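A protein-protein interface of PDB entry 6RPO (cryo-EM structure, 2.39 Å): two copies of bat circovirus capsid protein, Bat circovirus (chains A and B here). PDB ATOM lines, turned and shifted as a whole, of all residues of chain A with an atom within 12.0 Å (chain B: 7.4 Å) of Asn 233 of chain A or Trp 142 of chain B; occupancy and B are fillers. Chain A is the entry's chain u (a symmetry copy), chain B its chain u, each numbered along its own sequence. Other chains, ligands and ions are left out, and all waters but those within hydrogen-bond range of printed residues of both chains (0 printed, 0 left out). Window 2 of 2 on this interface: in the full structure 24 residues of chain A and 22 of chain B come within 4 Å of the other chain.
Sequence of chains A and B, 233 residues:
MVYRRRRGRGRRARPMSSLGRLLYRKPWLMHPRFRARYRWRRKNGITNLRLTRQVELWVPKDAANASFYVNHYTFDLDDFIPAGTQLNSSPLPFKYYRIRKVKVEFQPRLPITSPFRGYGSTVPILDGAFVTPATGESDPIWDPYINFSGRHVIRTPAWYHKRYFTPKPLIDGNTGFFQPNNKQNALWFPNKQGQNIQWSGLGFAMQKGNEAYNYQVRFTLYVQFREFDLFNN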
ATOM      1  N   THR A  85      13.614  16.058 -33.745  1.00  0.00           N
ATOM      2  CA  THR A  85      12.766  15.584 -34.825  1.00  0.00           C
ATOM      3  C   THR A  85      11.516  16.452 -34.937  1.00  0.00           C
ATOM      4  O   THR A  85      11.338  17.433 -34.208  1.00  0.00           O
ATOM      5  CB  THR A  85      12.390  14.118 -34.598  1.00  0.00           C
ATOM      6  OG1 THR A  85      11.979  13.934 -33.239  1.00  0.00           O
ATOM      7  CG2 THR A  85      13.562  13.209 -34.895  1.00  0.00           C
ATOM      8  N   GLN A  86      10.634  16.083 -35.865  1.00  0.00           N
ATOM      9  CA  GLN A  86       9.318  16.701 -35.945  1.00  0.00           C
ATOM     10  C   GLN A  86       8.440  16.268 -34.775  1.00  0.00           C
ATOM     11  O   GLN A  86       7.684  17.076 -34.227  1.00  0.00           O
ATOM     12  CB  GLN A  86       8.670  16.348 -37.288  1.00  0.00           C
ATOM     13  CG  GLN A  86       7.184  16.643 -37.410  1.00  0.00           C
ATOM     14  CD  GLN A  86       6.900  18.023 -37.966  1.00  0.00           C
ATOM     15  OE1 GLN A  86       7.570  18.995 -37.620  1.00  0.00           O
ATOM     16  NE2 GLN A  86       5.899  18.116 -38.831  1.00  0.00           N
ATOM     17  N   LEU A  87       8.561  15.005 -34.361  1.00  0.00           N
ATOM     18  CA  LEU A  87       7.773  14.486 -33.247  1.00  0.00           C
ATOM     19  C   LEU A  87       8.252  15.053 -31.914  1.00  0.00           C
ATOM     20  O   LEU A  87       7.486  15.690 -31.183  1.00  0.00           O
ATOM     21  CB  LEU A  87       7.834  12.957 -33.245  1.00  0.00           C
ATOM     22  CG  LEU A  87       7.061  12.210 -32.159  1.00  0.00           C
ATOM     23  CD1 LEU A  87       5.579  12.481 -32.267  1.00  0.00           C
ATOM     24  CD2 LEU A  87       7.348  10.722 -32.234  1.00  0.00           C
ATOM     25  N   ASN A  88       9.515  14.815 -31.573  1.00  0.00           N
ATOM     26  CA  ASN A  88      10.113  15.346 -30.352  1.00  0.00           C
ATOM     27  C   ASN A  88      11.114  16.428 -30.744  1.00  0.00           C
ATOM     28  O   ASN A  88      12.204  16.125 -31.236  1.00  0.00           O
ATOM     29  CB  ASN A  88      10.776  14.233 -29.544  1.00  0.00           C
ATOM     30  CG  ASN A  88       9.769  13.261 -28.951  1.00  0.00           C
ATOM     31  OD1 ASN A  88       9.097  13.570 -27.973  1.00  0.00           O
ATOM     32  ND2 ASN A  88       9.665  12.080 -29.541  1.00  0.00           N
ATOM     33  N   SER A  89      10.742  17.691 -30.520  1.00  0.00           N
ATOM     34  CA  SER A  89      11.513  18.810 -31.055  1.00  0.00           C
ATOM     35  C   SER A  89      12.841  19.000 -30.335  1.00  0.00           C
ATOM     36  O   SER A  89      13.808  19.468 -30.942  1.00  0.00           O
ATOM     37  CB  SER A  89      10.691  20.096 -30.981  1.00  0.00           C
ATOM     38  OG  SER A  89      10.477  20.489 -29.640  1.00  0.00           O
ATOM     39  N   PRO A  93      14.009  15.458 -23.643  1.00  0.00           N
ATOM     40  CA  PRO A  93      12.532  15.501 -23.588  1.00  0.00           C
ATOM     41  C   PRO A  93      11.995  16.035 -22.265  1.00  0.00           C
ATOM     42  O   PRO A  93      11.296  15.366 -21.508  1.00  0.00           O
ATOM     43  CB  PRO A  93      12.159  14.036 -23.835  1.00  0.00           C
ATOM     44  CG  PRO A  93      13.292  13.269 -23.264  1.00  0.00           C
ATOM     45  CD  PRO A  93      14.532  14.111 -23.366  1.00  0.00           C
ATOM     46  N   PHE A 228       9.296  15.861 -17.731  1.00  0.00           N
ATOM     47  CA  PHE A 228       9.496  14.860 -18.776  1.00  0.00           C
ATOM     48  C   PHE A 228       8.298  14.728 -19.719  1.00  0.00           C
ATOM     49  O   PHE A 228       7.182  14.453 -19.272  1.00  0.00           O
ATOM     50  CB  PHE A 228       9.806  13.517 -18.109  1.00  0.00           C
ATOM     51  CG  PHE A 228      10.094  12.408 -19.066  1.00  0.00           C
ATOM     52  CD1 PHE A 228      11.285  12.374 -19.769  1.00  0.00           C
ATOM     53  CD2 PHE A 228       9.180  11.382 -19.248  1.00  0.00           C
ATOM     54  CE1 PHE A 228      11.554  11.350 -20.653  1.00  0.00           C
ATOM     55  CE2 PHE A 228       9.446  10.350 -20.132  1.00  0.00           C
ATOM     56  CZ  PHE A 228      10.638  10.338 -20.834  1.00  0.00           C
ATOM     57  N   ASP A 229       8.509  14.943 -21.021  1.00  0.00           N
ATOM     58  CA  ASP A 229       7.452  14.814 -22.025  1.00  0.00           C
ATOM     59  C   ASP A 229       8.007  14.182 -23.299  1.00  0.00           C
ATOM     60  O   ASP A 229       8.500  14.873 -24.194  1.00  0.00           O
ATOM     61  CB  ASP A 229       6.780  16.166 -22.317  1.00  0.00           C
ATOM     62  CG  ASP A 229       7.775  17.294 -22.586  1.00  0.00           C
ATOM     63  OD1 ASP A 229       8.990  17.064 -22.470  1.00  0.00           O
ATOM     64  OD2 ASP A 229       7.335  18.406 -22.947  1.00  0.00           O
ATOM     65  N   LEU A 230       7.902  12.867 -23.404  1.00  0.00           N
ATOM     66  CA  LEU A 230       8.303  12.151 -24.607  1.00  0.00           C
ATOM     67  C   LEU A 230       7.042  11.750 -25.361  1.00  0.00           C
ATOM     68  O   LEU A 230       6.184  11.054 -24.811  1.00  0.00           O
ATOM     69  CB  LEU A 230       9.153  10.935 -24.251  1.00  0.00           C
ATOM     70  CG  LEU A 230       9.575  10.023 -25.400  1.00  0.00           C
ATOM     71  CD1 LEU A 230      10.637  10.691 -26.244  1.00  0.00           C
ATOM     72  CD2 LEU A 230      10.066   8.702 -24.863  1.00  0.00           C
ATOM     73  N   PHE A 231       6.912  12.203 -26.602  1.00  0.00           N
ATOM     74  CA  PHE A 231       5.808  11.767 -27.443  1.00  0.00           C
ATOM     75  C   PHE A 231       6.161  10.475 -28.170  1.00  0.00           C
ATOM     76  O   PHE A 231       7.239  10.336 -28.748  1.00  0.00           O
ATOM     77  CB  PHE A 231       5.433  12.848 -28.456  1.00  0.00           C
ATOM     78  CG  PHE A 231       5.088  14.167 -27.831  1.00  0.00           C
ATOM     79  CD1 PHE A 231       4.000  14.280 -26.981  1.00  0.00           C
ATOM     80  CD2 PHE A 231       5.857  15.291 -28.083  1.00  0.00           C
ATOM     81  CE1 PHE A 231       3.680  15.492 -26.399  1.00  0.00           C
ATOM     82  CE2 PHE A 231       5.543  16.505 -27.500  1.00  0.00           C
ATOM     83  CZ  PHE A 231       4.451  16.602 -26.659  1.00  0.00           C
ATOM     84  N   ASN A 232       5.235   9.519 -28.129  1.00  0.00           N
ATOM     85  CA  ASN A 232       5.408   8.232 -28.785  1.00  0.00           C
ATOM     86  C   ASN A 232       4.218   7.971 -29.698  1.00  0.00           C
ATOM     87  O   ASN A 232       3.074   8.267 -29.348  1.00  0.00           O
ATOM     88  CB  ASN A 232       5.555   7.090 -27.765  1.00  0.00           C
ATOM     89  CG  ASN A 232       5.834   5.745 -28.419  1.00  0.00           C
ATOM     90  OD1 ASN A 232       6.519   5.665 -29.435  1.00  0.00           O
ATOM     91  ND2 ASN A 232       5.307   4.682 -27.830  1.00  0.00           N
ATOM     92  N   ASN A 233       4.500   7.417 -30.871  1.00  0.00           N
ATOM     93  CA  ASN A 233       3.457   7.048 -31.821  1.00  0.00           C
ATOM     94  C   ASN A 233       2.990   5.616 -31.607  1.00  0.00           C
ATOM     95  O   ASN A 233       3.427   4.703 -32.303  1.00  0.00           O
ATOM     96  CB  ASN A 233       3.953   7.210 -33.251  1.00  0.00           C
ATOM     97  CG  ASN A 233       4.198   8.647 -33.613  1.00  0.00           C
ATOM     98  OD1 ASN A 233       3.414   9.525 -33.263  1.00  0.00           O
ATOM     99  ND2 ASN A 233       5.294   8.900 -34.317  1.00  0.00           N
ATOM    100  N   ALA B  66     -11.101   5.360 -32.742  1.00  0.00           N
ATOM    101  CA  ALA B  66     -10.843   5.663 -31.325  1.00  0.00           C
ATOM    102  C   ALA B  66      -9.783   6.753 -31.159  1.00  0.00           C
ATOM    103  O   ALA B  66      -8.802   6.596 -30.432  1.00  0.00           O
ATOM    104  CB  ALA B  66     -10.475   4.401 -30.533  1.00  0.00           C
ATOM    105  N   SER B  67      -9.996   7.874 -31.844  1.00  0.00           N
ATOM    106  CA  SER B  67      -9.086   9.005 -31.800  1.00  0.00           C
ATOM    107  C   SER B  67      -9.196   9.735 -30.462  1.00  0.00           C
ATOM    108  O   SER B  67      -9.991   9.384 -29.588  1.00  0.00           O
ATOM    109  CB  SER B  67      -9.369   9.955 -32.960  1.00  0.00           C
ATOM    110  OG  SER B  67      -8.497  11.066 -32.927  1.00  0.00           O
ATOM    111  N   PHE B  68      -8.393  10.777 -30.298  1.00  0.00           N
ATOM    112  CA  PHE B  68      -8.366  11.529 -29.058  1.00  0.00           C
ATOM    113  C   PHE B  68      -8.834  12.956 -29.292  1.00  0.00           C
ATOM    114  O   PHE B  68      -8.459  13.605 -30.269  1.00  0.00           O
ATOM    115  CB  PHE B  68      -6.967  11.530 -28.439  1.00  0.00           C
ATOM    116  CG  PHE B  68      -6.599  10.239 -27.782  1.00  0.00           C
ATOM    117  CD1 PHE B  68      -6.790  10.059 -26.421  1.00  0.00           C
ATOM    118  CD2 PHE B  68      -6.070   9.197 -28.527  1.00  0.00           C
ATOM    119  CE1 PHE B  68      -6.447   8.869 -25.815  1.00  0.00           C
ATOM    120  CE2 PHE B  68      -5.726   8.006 -27.927  1.00  0.00           C
ATOM    121  CZ  PHE B  68      -5.915   7.841 -26.572  1.00  0.00           C
ATOM    122  N   VAL B  70      -8.363  16.465 -28.022  1.00  0.00           N
ATOM    123  CA  VAL B  70      -7.344  17.194 -27.282  1.00  0.00           C
ATOM    124  C   VAL B  70      -7.739  18.660 -27.220  1.00  0.00           C
ATOM    125  O   VAL B  70      -7.934  19.304 -28.257  1.00  0.00           O
ATOM    126  CB  VAL B  70      -5.962  17.019 -27.935  1.00  0.00           C
ATOM    127  CG1 VAL B  70      -4.888  17.617 -27.063  1.00  0.00           C
ATOM    128  CG2 VAL B  70      -5.690  15.550 -28.199  1.00  0.00           C
ATOM    129  N   VAL B 131      -0.554  20.999 -26.608  1.00  0.00           N
ATOM    130  CA  VAL B 131      -0.358  20.185 -27.809  1.00  0.00           C
ATOM    131  C   VAL B 131      -1.612  20.213 -28.675  1.00  0.00           C
ATOM    132  O   VAL B 131      -1.733  19.437 -29.631  1.00  0.00           O
ATOM    133  CB  VAL B 131       0.029  18.734 -27.456  1.00  0.00           C
ATOM    134  CG1 VAL B 131       1.226  18.703 -26.527  1.00  0.00           C
ATOM    135  CG2 VAL B 131      -1.136  17.987 -26.838  1.00  0.00           C
ATOM    136  N   ASP B 139      -7.214  15.218 -35.329  1.00  0.00           N
ATOM    137  CA  ASP B 139      -7.127  14.661 -33.991  1.00  0.00           C
ATOM    138  C   ASP B 139      -6.254  13.405 -34.002  1.00  0.00           C
ATOM    139  O   ASP B 139      -6.452  12.524 -34.843  1.00  0.00           O
ATOM    140  CB  ASP B 139      -8.517  14.331 -33.465  1.00  0.00           C
ATOM    141  CG  ASP B 139      -9.314  15.575 -33.111  1.00  0.00           C
ATOM    142  OD1 ASP B 139      -8.691  16.599 -32.755  1.00  0.00           O
ATOM    143  OD2 ASP B 139     -10.562  15.531 -33.178  1.00  0.00           O
ATOM    144  N   PRO B 140      -5.291  13.302 -33.088  1.00  0.00           N
ATOM    145  CA  PRO B 140      -4.314  12.208 -33.151  1.00  0.00           C
ATOM    146  C   PRO B 140      -4.906  10.858 -32.768  1.00  0.00           C
ATOM    147  O   PRO B 140      -5.923  10.754 -32.080  1.00  0.00           O
ATOM    148  CB  PRO B 140      -3.239  12.637 -32.150  1.00  0.00           C
ATOM    149  CG  PRO B 140      -3.963  13.525 -31.193  1.00  0.00           C
ATOM    150  CD  PRO B 140      -4.981  14.259 -32.012  1.00  0.00           C
ATOM    151  N   ILE B 141      -4.236   9.803 -33.242  1.00  0.00           N
ATOM    152  CA  ILE B 141      -4.624   8.432 -32.931  1.00  0.00           C
ATOM    153  C   ILE B 141      -4.006   7.967 -31.614  1.00  0.00           C
ATOM    154  O   ILE B 141      -4.492   7.003 -31.007  1.00  0.00           O
ATOM    155  CB  ILE B 141      -4.231   7.538 -34.135  1.00  0.00           C
ATOM    156  CG1 ILE B 141      -4.753   8.140 -35.439  1.00  0.00           C
ATOM    157  CG2 ILE B 141      -4.813   6.127 -34.044  1.00  0.00           C
ATOM    158  CD1 ILE B 141      -6.259   8.239 -35.519  1.00  0.00           C
ATOM    159  N   TRP B 142      -3.012   8.686 -31.103  1.00  0.00           N
ATOM    160  CA  TRP B 142      -2.284   8.314 -29.899  1.00  0.00           C
ATOM    161  C   TRP B 142      -2.486   9.382 -28.832  1.00  0.00           C
ATOM    162  O   TRP B 142      -2.784  10.535 -29.142  1.00  0.00           O
ATOM    163  CB  TRP B 142      -0.777   8.125 -30.193  1.00  0.00           C
ATOM    164  CG  TRP B 142      -0.163   9.208 -31.058  1.00  0.00           C
ATOM    165  CD1 TRP B 142      -0.256   9.332 -32.416  1.00  0.00           C
ATOM    166  CD2 TRP B 142       0.646  10.306 -30.615  1.00  0.00           C
ATOM    167  NE1 TRP B 142       0.427  10.440 -32.839  1.00  0.00           N
ATOM    168  CE2 TRP B 142       0.992  11.056 -31.755  1.00  0.00           C
ATOM    169  CE3 TRP B 142       1.106  10.729 -29.365  1.00  0.00           C
ATOM    170  CZ2 TRP B 142       1.779  12.202 -31.683  1.00  0.00           C
ATOM    171  CZ3 TRP B 142       1.885  11.865 -29.296  1.00  0.00           C
ATOM    172  CH2 TRP B 142       2.216  12.589 -30.448  1.00  0.00           C
ATOM    173  N   ASP B 143      -2.329   8.982 -27.570  1.00  0.00           N
ATOM    174  CA  ASP B 143      -2.451   9.910 -26.446  1.00  0.00           C
ATOM    175  C   ASP B 143      -1.234  10.826 -26.399  1.00  0.00           C
ATOM    176  O   ASP B 143      -0.125  10.352 -26.133  1.00  0.00           O
ATOM    177  CB  ASP B 143      -2.576   9.143 -25.130  1.00  0.00           C
ATOM    178  CG  ASP B 143      -3.210   9.970 -24.003  1.00  0.00           C
ATOM    179  OD1 ASP B 143      -2.860  11.150 -23.815  1.00  0.00           O
ATOM    180  OD2 ASP B 143      -4.061   9.418 -23.280  1.00  0.00           O
ATOM    181  N   PRO B 144      -1.393  12.135 -26.615  1.00  0.00           N
ATOM    182  CA  PRO B 144      -0.231  13.028 -26.565  1.00  0.00           C
ATOM    183  C   PRO B 144       0.259  13.336 -25.159  1.00  0.00           C
ATOM    184  O   PRO B 144       1.362  13.873 -25.016  1.00  0.00           O
ATOM    185  CB  PRO B 144      -0.741  14.294 -27.261  1.00  0.00           C
ATOM    186  CG  PRO B 144      -2.199  14.302 -26.974  1.00  0.00           C
ATOM    187  CD  PRO B 144      -2.649  12.872 -26.838  1.00  0.00           C
ATOM    188  N   TYR B 145      -0.507  13.009 -24.125  1.00  0.00           N
ATOM    189  CA  TYR B 145      -0.139  13.324 -22.754  1.00  0.00           C
ATOM    190  C   TYR B 145       0.181  12.103 -21.909  1.00  0.00           C
ATOM    191  O   TYR B 145       0.219  12.222 -20.684  1.00  0.00           O
ATOM    192  CB  TYR B 145      -1.263  14.099 -22.075  1.00  0.00           C
ATOM    193  CG  TYR B 145      -1.420  15.505 -22.562  1.00  0.00           C
ATOM    194  CD1 TYR B 145      -0.311  16.311 -22.787  1.00  0.00           C
ATOM    195  CD2 TYR B 145      -2.679  16.031 -22.796  1.00  0.00           C
ATOM    196  CE1 TYR B 145      -0.464  17.608 -23.230  1.00  0.00           C
ATOM    197  CE2 TYR B 145      -2.839  17.317 -23.236  1.00  0.00           C
ATOM    198  CZ  TYR B 145      -1.734  18.107 -23.440  1.00  0.00           C
ATOM    199  OH  TYR B 145      -1.904  19.392 -23.891  1.00  0.00           O
ATOM    200  N   ILE B 146       0.417  10.940 -22.517  1.00  0.00           N
ATOM    201  CA  ILE B 146       0.491   9.723 -21.718  1.00  0.00           C
ATOM    202  C   ILE B 146       1.826   9.592 -20.981  1.00  0.00           C
ATOM    203  O   ILE B 146       1.874   8.960 -19.923  1.00  0.00           O
ATOM    204  CB  ILE B 146       0.176   8.490 -22.596  1.00  0.00           C
ATOM    205  CG1 ILE B 146      -0.350   7.340 -21.730  1.00  0.00           C
ATOM    206  CG2 ILE B 146       1.374   8.056 -23.436  1.00  0.00           C
ATOM    207  CD1 ILE B 146      -0.770   6.123 -22.503  1.00  0.00           C
ATOM    208  N   ASN B 147       2.894  10.226 -21.462  1.00  0.00           N
ATOM    209  CA  ASN B 147       4.201  10.108 -20.831  1.00  0.00           C
ATOM    210  C   ASN B 147       4.553  11.285 -19.937  1.00  0.00           C
ATOM    211  O   ASN B 147       5.679  11.344 -19.444  1.00  0.00           O
ATOM    212  CB  ASN B 147       5.295   9.948 -21.887  1.00  0.00           C
ATOM    213  CG  ASN B 147       5.374   8.552 -22.438  1.00  0.00           C
ATOM    214  OD1 ASN B 147       5.235   7.574 -21.711  1.00  0.00           O
ATOM    215  ND2 ASN B 147       5.595   8.449 -23.737  1.00  0.00           N
ATOM    216  N   ALA B 205      -6.759  15.036 -22.880  1.00  0.00           N
ATOM    217  CA  ALA B 205      -7.020  14.243 -24.075  1.00  0.00           C
ATOM    218  C   ALA B 205      -8.072  13.213 -23.702  1.00  0.00           C
ATOM    219  O   ALA B 205      -7.940  12.548 -22.674  1.00  0.00           O
ATOM    220  CB  ALA B 205      -5.748  13.573 -24.592  1.00  0.00           C
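NE1 of Trp 142 of chain B is in hydrogen-bond range of OD1 of Asn 233 of chain A, 3.2 Å away. The backbone carbonyl oxygen (O) of Phe 228 of chain A lies close to the backbone carbonyl oxygen (O) of Asn 147 of chain B, at 3.5 Å. The side-chain amide nitrogen (ND2) of Asn 147 of chain B sits at hydrogen-bond distance from the backbone carbonyl oxygen (O) of Leu 230 of chain A, at 2.9 Å.
The backbone NH (N) of Val 131 of chain B lies close to the side-chain hydroxyl (OH) of Tyr 145 of chain B (3.4 Å). OD1 of Asn 88 of chain A sits at hydrogen-bond distance from N of Phe 231 of chain A, at 2.9 Å.
Among the printed residues, pairs that only touch across the chains: Leu 87 of chain A with Trp 142 of chain B, Phe 231 of chain A with Val 131 of chain B, Phe 231 of chain A with Trp 142 of chain B, Phe 231 of chain A with Pro 144 of chain B and Asn 232 of chain A with Trp 142 of chain B.
Printed residues of chain B within 4 Å of Leu 230 of chain A: Asn 147. No residue of chain A comes within 4 Å of Ser 67 of chain B. No residue of chain A comes within 4 Å of Phe 68 of chain B. Printed residues of chain A within 4 Å of Val 131 of chain B: Phe 231. Asp 139 of chain B touches none of the printed residues of chain A. No residue of chain A comes within 4 Å of Pro 140 of chain B. Of chain A, only Leu 87, Phe 231, Asn 232 and Asn 233 come within 4 Å of Trp 142 of chain B. The nearest residue of chain A that does not touch Trp 142 of chain B is Leu 230 of chain A (6.3 Å). The nearest printed residue of chain B that does not touch Phe 228 of chain A is Ile 146 of chain B (7.4 Å).
Of the 12 printed residues of chain A, 6 touch a printed residue of chain B. Printed residues of chain A that touch a printed residue of chain B: Leu 87, Phe 228, Leu 230, Phe 231, Asn 232 and Asn 233. Among the printed residues, 8 pairs touch across the chains. Among the printed residues, no Asp or Glu carboxylate lies within 4 Å of a Lys or Arg side-chain nitrogen of the other chain.
No position is printed for both chains. Of the 8 pairs that touch across the chains among the printed residues, none has its exchanged pair printed and touching as well.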
